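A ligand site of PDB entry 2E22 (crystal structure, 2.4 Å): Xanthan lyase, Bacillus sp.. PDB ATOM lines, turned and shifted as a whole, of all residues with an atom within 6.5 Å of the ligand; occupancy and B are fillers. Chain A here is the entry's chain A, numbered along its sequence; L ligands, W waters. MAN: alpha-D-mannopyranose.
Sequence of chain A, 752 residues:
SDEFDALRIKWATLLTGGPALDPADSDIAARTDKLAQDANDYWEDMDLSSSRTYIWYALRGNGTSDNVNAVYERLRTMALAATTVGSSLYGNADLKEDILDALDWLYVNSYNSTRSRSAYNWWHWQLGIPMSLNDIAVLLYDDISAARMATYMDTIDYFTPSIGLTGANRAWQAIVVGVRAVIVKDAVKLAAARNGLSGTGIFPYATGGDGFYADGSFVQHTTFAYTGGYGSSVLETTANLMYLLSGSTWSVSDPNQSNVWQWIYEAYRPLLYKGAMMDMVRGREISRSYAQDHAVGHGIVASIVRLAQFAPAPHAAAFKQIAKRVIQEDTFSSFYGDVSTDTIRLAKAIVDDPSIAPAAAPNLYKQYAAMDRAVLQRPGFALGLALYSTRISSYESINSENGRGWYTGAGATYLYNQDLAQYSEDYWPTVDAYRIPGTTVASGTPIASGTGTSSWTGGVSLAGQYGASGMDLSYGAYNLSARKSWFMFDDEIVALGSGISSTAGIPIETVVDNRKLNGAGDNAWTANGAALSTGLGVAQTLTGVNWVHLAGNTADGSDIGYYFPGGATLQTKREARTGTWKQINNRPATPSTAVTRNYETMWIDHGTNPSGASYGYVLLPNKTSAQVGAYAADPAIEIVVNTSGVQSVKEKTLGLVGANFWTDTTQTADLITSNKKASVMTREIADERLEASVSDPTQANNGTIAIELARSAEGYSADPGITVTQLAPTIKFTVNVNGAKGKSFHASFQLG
OH of Tyr 230 is in hydrogen-bond range of NH1 of Arg 284 (3.0 Å).
The side-chain hydroxyl of Tyr 230 lies close to a ring nitrogen (NE2) of His 221, at 3.2 Å.
The side-chain carboxylate of Glu 401 lies within salt-bridge range of the guanidinium group of Arg 284, 2.7 Å away.
The side-chain hydroxyl (OH) of Tyr 226 lies within hydrogen-bond range of the backbone NH (N) of Arg 284 (3.1 Å).
NH1 of Arg 288 is in salt-bridge range of OE1 of Glu 285 (3.9 Å).
The guanidinium group (NE) of Arg 288 is in salt-bridge range of the side-chain carboxylate (OE2) of Glu 401 (2.8 Å).
The guanidinium group (NH2) of Arg 587 lies within hydrogen-bond range of the side-chain hydroxyl (OH) of Tyr 290, 3.3 Å away.
The backbone NH of Trp 123 lies close to the side-chain amide nitrogen of Asn 121 (3.2 Å).
CE3 of Trp 123 touches C6 of the ligand (3.4 Å).
His 124 touches the ligand (NE2 to C6, 3.9 Å).
Six residues have an atom within 4 Å of the ligand: Trp 123, His 124, Tyr 230, Arg 284, Arg 288 and Arg 587.
The nearest printed residue that does not touch the ligand is Trp 172 (4.1 Å).
An oxygen (O1) of the ligand is in hydrogen-bond range of the side-chain hydroxyl (OH) of Tyr 230 (2.7 Å).
NH2 of Arg 284 lies within hydrogen-bond range of O2 of the ligand, 2.9 Å away.
The guanidinium group (NH2) of Arg 288 lies within hydrogen-bond range of an oxygen (O2) of the ligand.
The guanidinium group of Arg 587 lies within hydrogen-bond range of an oxygen (O6) of the ligand, 3.3 Å away.
Water W2 bridges an oxygen (O2) of the ligand (2.6 Å) and the side-chain carboxylate of Glu 285 (2.7 Å).
Water W4 lies within hydrogen-bond range of an oxygen (O3) of the ligand (2.8 Å), the side-chain hydroxyl of Ser 233 (3.0 Å) and the side-chain carboxylate of Glu 285 (3.0 Å).
Water W1 lies within hydrogen-bond range of O5 of the ligand (2.9 Å) and OD1 of Asn 121 (2.9 Å).
Water W3 lies within hydrogen-bond range of an oxygen (O4) of the ligand and the side-chain hydroxyl of Tyr 290.
Water W6 bridges NE2 of His 124 (3.0 Å) and O6 of the ligand (3.4 Å).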
ATOM      1  N   ASP A  66      14.146 -21.706  24.368  1.00  0.00           N
ATOM      2  CA  ASP A  66      13.479 -20.886  25.369  1.00  0.00           C
ATOM      3  C   ASP A  66      14.284 -20.754  26.655  1.00  0.00           C
ATOM      4  O   ASP A  66      14.589 -19.656  27.107  1.00  0.00           O
ATOM      5  CB  ASP A  66      12.098 -21.453  25.687  1.00  0.00           C
ATOM      6  CG  ASP A  66      11.133 -21.291  24.546  1.00  0.00           C
ATOM      7  OD1 ASP A  66      11.458 -21.718  23.427  1.00  0.00           O
ATOM      8  OD2 ASP A  66      10.028 -20.738  24.780  1.00  0.00           O
ATOM      9  N   ASN A 121      14.654 -23.406  18.318  1.00  0.00           N
ATOM     10  CA  ASN A 121      14.131 -22.320  17.488  1.00  0.00           C
ATOM     11  C   ASN A 121      15.311 -21.485  16.997  1.00  0.00           C
ATOM     12  O   ASN A 121      16.068 -20.939  17.797  1.00  0.00           O
ATOM     13  CB  ASN A 121      13.177 -21.459  18.331  1.00  0.00           C
ATOM     14  CG  ASN A 121      12.527 -20.356  17.522  1.00  0.00           C
ATOM     15  OD1 ASN A 121      11.683 -19.618  18.041  1.00  0.00           O
ATOM     16  ND2 ASN A 121      12.897 -20.241  16.256  1.00  0.00           N
ATOM     17  N   TRP A 122      15.453 -21.390  15.681  1.00  0.00           N
ATOM     18  CA  TRP A 122      16.557 -20.639  15.069  1.00  0.00           C
ATOM     19  C   TRP A 122      16.689 -19.211  15.573  1.00  0.00           C
ATOM     20  O   TRP A 122      17.802 -18.704  15.744  1.00  0.00           O
ATOM     21  CB  TRP A 122      16.414 -20.608  13.542  1.00  0.00           C
ATOM     22  CG  TRP A 122      15.360 -19.666  13.072  1.00  0.00           C
ATOM     23  CD1 TRP A 122      14.033 -19.938  12.886  1.00  0.00           C
ATOM     24  CD2 TRP A 122      15.523 -18.268  12.819  1.00  0.00           C
ATOM     25  NE1 TRP A 122      13.358 -18.794  12.536  1.00  0.00           N
ATOM     26  CE2 TRP A 122      14.249 -17.748  12.484  1.00  0.00           C
ATOM     27  CE3 TRP A 122      16.624 -17.397  12.849  1.00  0.00           C
ATOM     28  CZ2 TRP A 122      14.044 -16.408  12.178  1.00  0.00           C
ATOM     29  CZ3 TRP A 122      16.415 -16.065  12.544  1.00  0.00           C
ATOM     30  CH2 TRP A 122      15.134 -15.576  12.213  1.00  0.00           C
ATOM     31  N   TRP A 123      15.568 -18.545  15.800  1.00  0.00           N
ATOM     32  CA  TRP A 123      15.580 -17.175  16.258  1.00  0.00           C
ATOM     33  C   TRP A 123      16.424 -16.990  17.512  1.00  0.00           C
ATOM     34  O   TRP A 123      17.209 -16.054  17.611  1.00  0.00           O
ATOM     35  CB  TRP A 123      14.149 -16.687  16.524  1.00  0.00           C
ATOM     36  CG  TRP A 123      14.085 -15.214  16.732  1.00  0.00           C
ATOM     37  CD1 TRP A 123      14.008 -14.255  15.765  1.00  0.00           C
ATOM     38  CD2 TRP A 123      14.163 -14.526  17.982  1.00  0.00           C
ATOM     39  NE1 TRP A 123      14.036 -13.000  16.343  1.00  0.00           N
ATOM     40  CE2 TRP A 123      14.139 -13.144  17.702  1.00  0.00           C
ATOM     41  CE3 TRP A 123      14.257 -14.938  19.316  1.00  0.00           C
ATOM     42  CZ2 TRP A 123      14.205 -12.169  18.706  1.00  0.00           C
ATOM     43  CZ3 TRP A 123      14.327 -13.976  20.320  1.00  0.00           C
ATOM     44  CH2 TRP A 123      14.291 -12.606  20.002  1.00  0.00           C
ATOM     45  N   HIS A 124      16.246 -17.886  18.477  1.00  0.00           N
ATOM     46  CA  HIS A 124      16.974 -17.820  19.741  1.00  0.00           C
ATOM     47  C   HIS A 124      18.490 -17.951  19.593  1.00  0.00           C
ATOM     48  O   HIS A 124      19.246 -17.165  20.178  1.00  0.00           O
ATOM     49  CB  HIS A 124      16.462 -18.903  20.688  1.00  0.00           C
ATOM     50  CG  HIS A 124      15.136 -18.586  21.296  1.00  0.00           C
ATOM     51  ND1 HIS A 124      14.181 -19.545  21.555  1.00  0.00           N
ATOM     52  CD2 HIS A 124      14.610 -17.406  21.722  1.00  0.00           C
ATOM     53  CE1 HIS A 124      13.126 -18.973  22.105  1.00  0.00           C
ATOM     54  NE2 HIS A 124      13.365 -17.679  22.215  1.00  0.00           N
ATOM     55  N   ASN A 169      13.612  -9.212  11.165  1.00  0.00           N
ATOM     56  CA  ASN A 169      14.727 -10.146  11.238  1.00  0.00           C
ATOM     57  C   ASN A 169      16.022  -9.539  10.686  1.00  0.00           C
ATOM     58  O   ASN A 169      17.080  -9.673  11.310  1.00  0.00           O
ATOM     59  CB  ASN A 169      14.385 -11.449  10.514  1.00  0.00           C
ATOM     60  CG  ASN A 169      13.214 -12.181  11.147  1.00  0.00           C
ATOM     61  OD1 ASN A 169      13.142 -12.334  12.365  1.00  0.00           O
ATOM     62  ND2 ASN A 169      12.277 -12.630  10.319  1.00  0.00           N
ATOM     63  N   TRP A 172      17.318  -7.124  13.103  1.00  0.00           N
ATOM     64  CA  TRP A 172      17.910  -7.819  14.244  1.00  0.00           C
ATOM     65  C   TRP A 172      19.317  -8.300  13.941  1.00  0.00           C
ATOM     66  O   TRP A 172      20.193  -8.218  14.801  1.00  0.00           O
ATOM     67  CB  TRP A 172      17.051  -9.009  14.679  1.00  0.00           C
ATOM     68  CG  TRP A 172      15.943  -8.626  15.621  1.00  0.00           C
ATOM     69  CD1 TRP A 172      16.015  -7.771  16.685  1.00  0.00           C
ATOM     70  CD2 TRP A 172      14.597  -9.124  15.601  1.00  0.00           C
ATOM     71  NE1 TRP A 172      14.810  -7.712  17.336  1.00  0.00           N
ATOM     72  CE2 TRP A 172      13.911  -8.532  16.697  1.00  0.00           C
ATOM     73  CE3 TRP A 172      13.889 -10.017  14.773  1.00  0.00           C
ATOM     74  CZ2 TRP A 172      12.572  -8.803  16.982  1.00  0.00           C
ATOM     75  CZ3 TRP A 172      12.555 -10.279  15.057  1.00  0.00           C
ATOM     76  CH2 TRP A 172      11.911  -9.676  16.154  1.00  0.00           C
ATOM     77  N   HIS A 221       5.855 -11.362   7.690  1.00  0.00           N
ATOM     78  CA  HIS A 221       5.406 -12.720   7.408  1.00  0.00           C
ATOM     79  C   HIS A 221       4.440 -12.730   6.221  1.00  0.00           C
ATOM     80  O   HIS A 221       3.468 -13.479   6.179  1.00  0.00           O
ATOM     81  CB  HIS A 221       4.740 -13.349   8.637  1.00  0.00           C
ATOM     82  CG  HIS A 221       5.705 -13.733   9.706  1.00  0.00           C
ATOM     83  ND1 HIS A 221       5.331 -14.404  10.848  1.00  0.00           N
ATOM     84  CD2 HIS A 221       7.043 -13.527   9.824  1.00  0.00           C
ATOM     85  CE1 HIS A 221       6.387 -14.592  11.619  1.00  0.00           C
ATOM     86  NE2 HIS A 221       7.441 -14.067  11.014  1.00  0.00           N
ATOM     87  N   TYR A 226       1.264  -5.889  10.988  1.00  0.00           N
ATOM     88  CA  TYR A 226       2.133  -6.001  12.161  1.00  0.00           C
ATOM     89  C   TYR A 226       2.813  -4.767  12.731  1.00  0.00           C
ATOM     90  O   TYR A 226       3.773  -4.895  13.473  1.00  0.00           O
ATOM     91  CB  TYR A 226       3.207  -7.049  11.864  1.00  0.00           C
ATOM     92  CG  TYR A 226       3.027  -8.342  12.630  1.00  0.00           C
ATOM     93  CD1 TYR A 226       2.965  -8.339  14.025  1.00  0.00           C
ATOM     94  CD2 TYR A 226       2.904  -9.562  11.953  1.00  0.00           C
ATOM     95  CE1 TYR A 226       2.784  -9.525  14.741  1.00  0.00           C
ATOM     96  CE2 TYR A 226       2.721 -10.749  12.659  1.00  0.00           C
ATOM     97  CZ  TYR A 226       2.668 -10.728  14.051  1.00  0.00           C
ATOM     98  OH  TYR A 226       2.487 -11.893  14.755  1.00  0.00           O
ATOM     99  N   GLY A 229       3.559  -5.151  16.333  1.00  0.00           N
ATOM    100  CA  GLY A 229       4.271  -6.349  16.763  1.00  0.00           C
ATOM    101  C   GLY A 229       5.698  -6.335  16.241  1.00  0.00           C
ATOM    102  O   GLY A 229       6.580  -5.740  16.872  1.00  0.00           O
ATOM    103  N   TYR A 230       5.945  -6.967  15.092  1.00  0.00           N
ATOM    104  CA  TYR A 230       7.284  -6.972  14.515  1.00  0.00           C
ATOM    105  C   TYR A 230       7.666  -5.541  14.171  1.00  0.00           C
ATOM    106  O   TYR A 230       8.847  -5.183  14.181  1.00  0.00           O
ATOM    107  CB  TYR A 230       7.324  -7.834  13.250  1.00  0.00           C
ATOM    108  CG  TYR A 230       7.372  -9.328  13.504  1.00  0.00           C
ATOM    109  CD1 TYR A 230       8.518  -9.927  14.031  1.00  0.00           C
ATOM    110  CD2 TYR A 230       6.278 -10.135  13.214  1.00  0.00           C
ATOM    111  CE1 TYR A 230       8.571 -11.311  14.265  1.00  0.00           C
ATOM    112  CE2 TYR A 230       6.316 -11.524  13.441  1.00  0.00           C
ATOM    113  CZ  TYR A 230       7.463 -12.100  13.965  1.00  0.00           C
ATOM    114  OH  TYR A 230       7.486 -13.455  14.202  1.00  0.00           O
ATOM    115  N   SER A 233       9.488  -3.839  16.988  1.00  0.00           N
ATOM    116  CA  SER A 233      10.863  -4.286  17.024  1.00  0.00           C
ATOM    117  C   SER A 233      11.716  -3.629  15.954  1.00  0.00           C
ATOM    118  O   SER A 233      12.847  -3.231  16.223  1.00  0.00           O
ATOM    119  CB  SER A 233      10.920  -5.802  16.872  1.00  0.00           C
ATOM    120  OG  SER A 233      10.194  -6.418  17.927  1.00  0.00           O
ATOM    121  N   ARG A 284       0.049 -11.830  16.677  1.00  0.00           N
ATOM    122  CA  ARG A 284      -0.037 -12.845  17.728  1.00  0.00           C
ATOM    123  C   ARG A 284       0.465 -12.390  19.079  1.00  0.00           C
ATOM    124  O   ARG A 284       0.292 -13.085  20.076  1.00  0.00           O
ATOM    125  CB  ARG A 284       0.711 -14.125  17.314  1.00  0.00           C
ATOM    126  CG  ARG A 284       2.233 -14.069  17.372  1.00  0.00           C
ATOM    127  CD  ARG A 284       2.824 -15.440  17.064  1.00  0.00           C
ATOM    128  NE  ARG A 284       4.244 -15.554  17.400  1.00  0.00           N
ATOM    129  CZ  ARG A 284       5.255 -15.112  16.657  1.00  0.00           C
ATOM    130  NH1 ARG A 284       5.017 -14.505  15.494  1.00  0.00           N
ATOM    131  NH2 ARG A 284       6.507 -15.269  17.066  1.00  0.00           N
ATOM    132  N   GLU A 285       1.061 -11.207  19.117  1.00  0.00           N
ATOM    133  CA  GLU A 285       1.595 -10.696  20.365  1.00  0.00           C
ATOM    134  C   GLU A 285       0.569 -10.295  21.403  1.00  0.00           C
ATOM    135  O   GLU A 285       0.905 -10.083  22.570  1.00  0.00           O
ATOM    136  CB  GLU A 285       2.547  -9.540  20.090  1.00  0.00           C
ATOM    137  CG  GLU A 285       3.843 -10.006  19.469  1.00  0.00           C
ATOM    138  CD  GLU A 285       4.795  -8.887  19.186  1.00  0.00           C
ATOM    139  OE1 GLU A 285       4.908  -7.978  20.035  1.00  0.00           O
ATOM    140  OE2 GLU A 285       5.443  -8.916  18.120  1.00  0.00           O
ATOM    141  N   ARG A 288       0.529 -12.182  24.672  1.00  0.00           N
ATOM    142  CA  ARG A 288       1.633 -12.070  25.633  1.00  0.00           C
ATOM    143  C   ARG A 288       1.279 -11.166  26.796  1.00  0.00           C
ATOM    144  O   ARG A 288       1.021  -9.966  26.634  1.00  0.00           O
ATOM    145  CB  ARG A 288       2.880 -11.549  24.914  1.00  0.00           C
ATOM    146  CG  ARG A 288       3.317 -12.480  23.799  1.00  0.00           C
ATOM    147  CD  ARG A 288       4.437 -11.894  22.974  1.00  0.00           C
ATOM    148  NE  ARG A 288       4.924 -12.872  22.018  1.00  0.00           N
ATOM    149  CZ  ARG A 288       5.877 -12.635  21.120  1.00  0.00           C
ATOM    150  NH1 ARG A 288       6.441 -11.429  21.060  1.00  0.00           N
ATOM    151  NH2 ARG A 288       6.264 -13.590  20.292  1.00  0.00           N
ATOM    152  N   TYR A 290       3.132 -10.041  29.108  1.00  0.00           N
ATOM    153  CA  TYR A 290       4.109  -8.989  29.356  1.00  0.00           C
ATOM    154  C   TYR A 290       4.085  -7.887  28.317  1.00  0.00           C
ATOM    155  O   TYR A 290       4.779  -6.879  28.465  1.00  0.00           O
ATOM    156  CB  TYR A 290       5.528  -9.569  29.437  1.00  0.00           C
ATOM    157  CG  TYR A 290       5.931 -10.381  28.237  1.00  0.00           C
ATOM    158  CD1 TYR A 290       5.648 -11.736  28.160  1.00  0.00           C
ATOM    159  CD2 TYR A 290       6.600  -9.781  27.173  1.00  0.00           C
ATOM    160  CE1 TYR A 290       6.030 -12.485  27.049  1.00  0.00           C
ATOM    161  CE2 TYR A 290       6.977 -10.515  26.062  1.00  0.00           C
ATOM    162  CZ  TYR A 290       6.689 -11.864  26.005  1.00  0.00           C
ATOM    163  OH  TYR A 290       7.091 -12.600  24.900  1.00  0.00           O
ATOM    164  N   ILE A 398       1.317 -19.135  15.763  1.00  0.00           N
ATOM    165  CA  ILE A 398       2.424 -20.079  15.624  1.00  0.00           C
ATOM    166  C   ILE A 398       3.119 -20.166  16.969  1.00  0.00           C
ATOM    167  O   ILE A 398       2.905 -19.323  17.848  1.00  0.00           O
ATOM    168  CB  ILE A 398       3.426 -19.602  14.544  1.00  0.00           C
ATOM    169  CG1 ILE A 398       4.018 -18.260  14.925  1.00  0.00           C
ATOM    170  CG2 ILE A 398       2.733 -19.493  13.198  1.00  0.00           C
ATOM    171  CD1 ILE A 398       4.994 -17.722  13.905  1.00  0.00           C
ATOM    172  N   ASN A 399       3.938 -21.206  17.132  1.00  0.00           N
ATOM    173  CA  ASN A 399       4.675 -21.439  18.380  1.00  0.00           C
ATOM    174  C   ASN A 399       3.778 -21.412  19.612  1.00  0.00           C
ATOM    175  O   ASN A 399       4.155 -20.886  20.652  1.00  0.00           O
ATOM    176  CB  ASN A 399       5.786 -20.398  18.535  1.00  0.00           C
ATOM    177  CG  ASN A 399       6.738 -20.400  17.353  1.00  0.00           C
ATOM    178  OD1 ASN A 399       7.133 -21.450  16.857  1.00  0.00           O
ATOM    179  ND2 ASN A 399       7.109 -19.204  16.899  1.00  0.00           N
ATOM    180  N   GLU A 401       1.165 -19.713  20.220  1.00  0.00           N
ATOM    181  CA  GLU A 401       0.730 -18.371  20.605  1.00  0.00           C
ATOM    182  C   GLU A 401      -0.523 -17.927  19.856  1.00  0.00           C
ATOM    183  O   GLU A 401      -0.659 -18.211  18.661  1.00  0.00           O
ATOM    184  CB  GLU A 401       1.846 -17.353  20.334  1.00  0.00           C
ATOM    185  CG  GLU A 401       3.076 -17.520  21.185  1.00  0.00           C
ATOM    186  CD  GLU A 401       4.026 -16.368  21.012  1.00  0.00           C
ATOM    187  OE1 GLU A 401       4.687 -16.276  19.953  1.00  0.00           O
ATOM    188  OE2 GLU A 401       4.117 -15.535  21.953  1.00  0.00           O
ATOM    189  N   ARG A 587       3.319 -21.466  26.215  1.00  0.00           N
ATOM    190  CA  ARG A 587       4.787 -21.548  26.305  1.00  0.00           C
ATOM    191  C   ARG A 587       5.221 -21.569  27.770  1.00  0.00           C
ATOM    192  O   ARG A 587       4.497 -21.098  28.658  1.00  0.00           O
ATOM    193  CB  ARG A 587       5.421 -20.349  25.602  1.00  0.00           C
ATOM    194  CG  ARG A 587       5.336 -20.419  24.084  1.00  0.00           C
ATOM    195  CD  ARG A 587       6.075 -19.279  23.389  1.00  0.00           C
ATOM    196  NE  ARG A 587       5.718 -17.954  23.915  1.00  0.00           N
ATOM    197  CZ  ARG A 587       6.371 -16.822  23.601  1.00  0.00           C
ATOM    198  NH1 ARG A 587       7.416 -16.836  22.760  1.00  0.00           N
ATOM    199  NH2 ARG A 587       6.053 -15.619  24.091  1.00  0.00           N
HETATM  200  C1  MAN L   1       9.993 -13.560  17.099  1.00  0.00           C
HETATM  201  C2  MAN L   1       9.157 -12.394  17.630  1.00  0.00           C
HETATM  202  C3  MAN L   1       9.798 -11.824  18.896  1.00  0.00           C
HETATM  203  C4  MAN L   1      10.019 -12.946  19.924  1.00  0.00           C
HETATM  204  C5  MAN L   1      10.820 -14.090  19.285  1.00  0.00           C
HETATM  205  C6  MAN L   1      10.993 -15.273  20.214  1.00  0.00           C
HETATM  206  O1  MAN L   1       9.363 -14.127  16.005  1.00  0.00           O
HETATM  207  O2  MAN L   1       7.831 -12.844  17.929  1.00  0.00           O
HETATM  208  O3  MAN L   1       8.959 -10.826  19.452  1.00  0.00           O
HETATM  209  O4  MAN L   1      10.735 -12.436  21.039  1.00  0.00           O
HETATM  210  O5  MAN L   1      10.135 -14.573  18.100  1.00  0.00           O
HETATM  211  O6  MAN L   1       9.780 -15.605  20.870  1.00  0.00           O
HETATM  212  O   HOH W   1      10.283 -17.258  17.067  1.00  0.00           O
HETATM  213  O   HOH W   2       6.310 -11.110  16.787  1.00  0.00           O
HETATM  214  O   HOH W   3       9.291 -10.589  23.255  1.00  0.00           O
HETATM  215  O   HOH W   4       8.403  -8.757  17.605  1.00  0.00           O
HETATM  216  O   HOH W   5       7.440 -16.983  19.530  1.00  0.00           O
HETATM  217  O   HOH W   6      11.371 -16.108  23.837  1.00  0.00           O
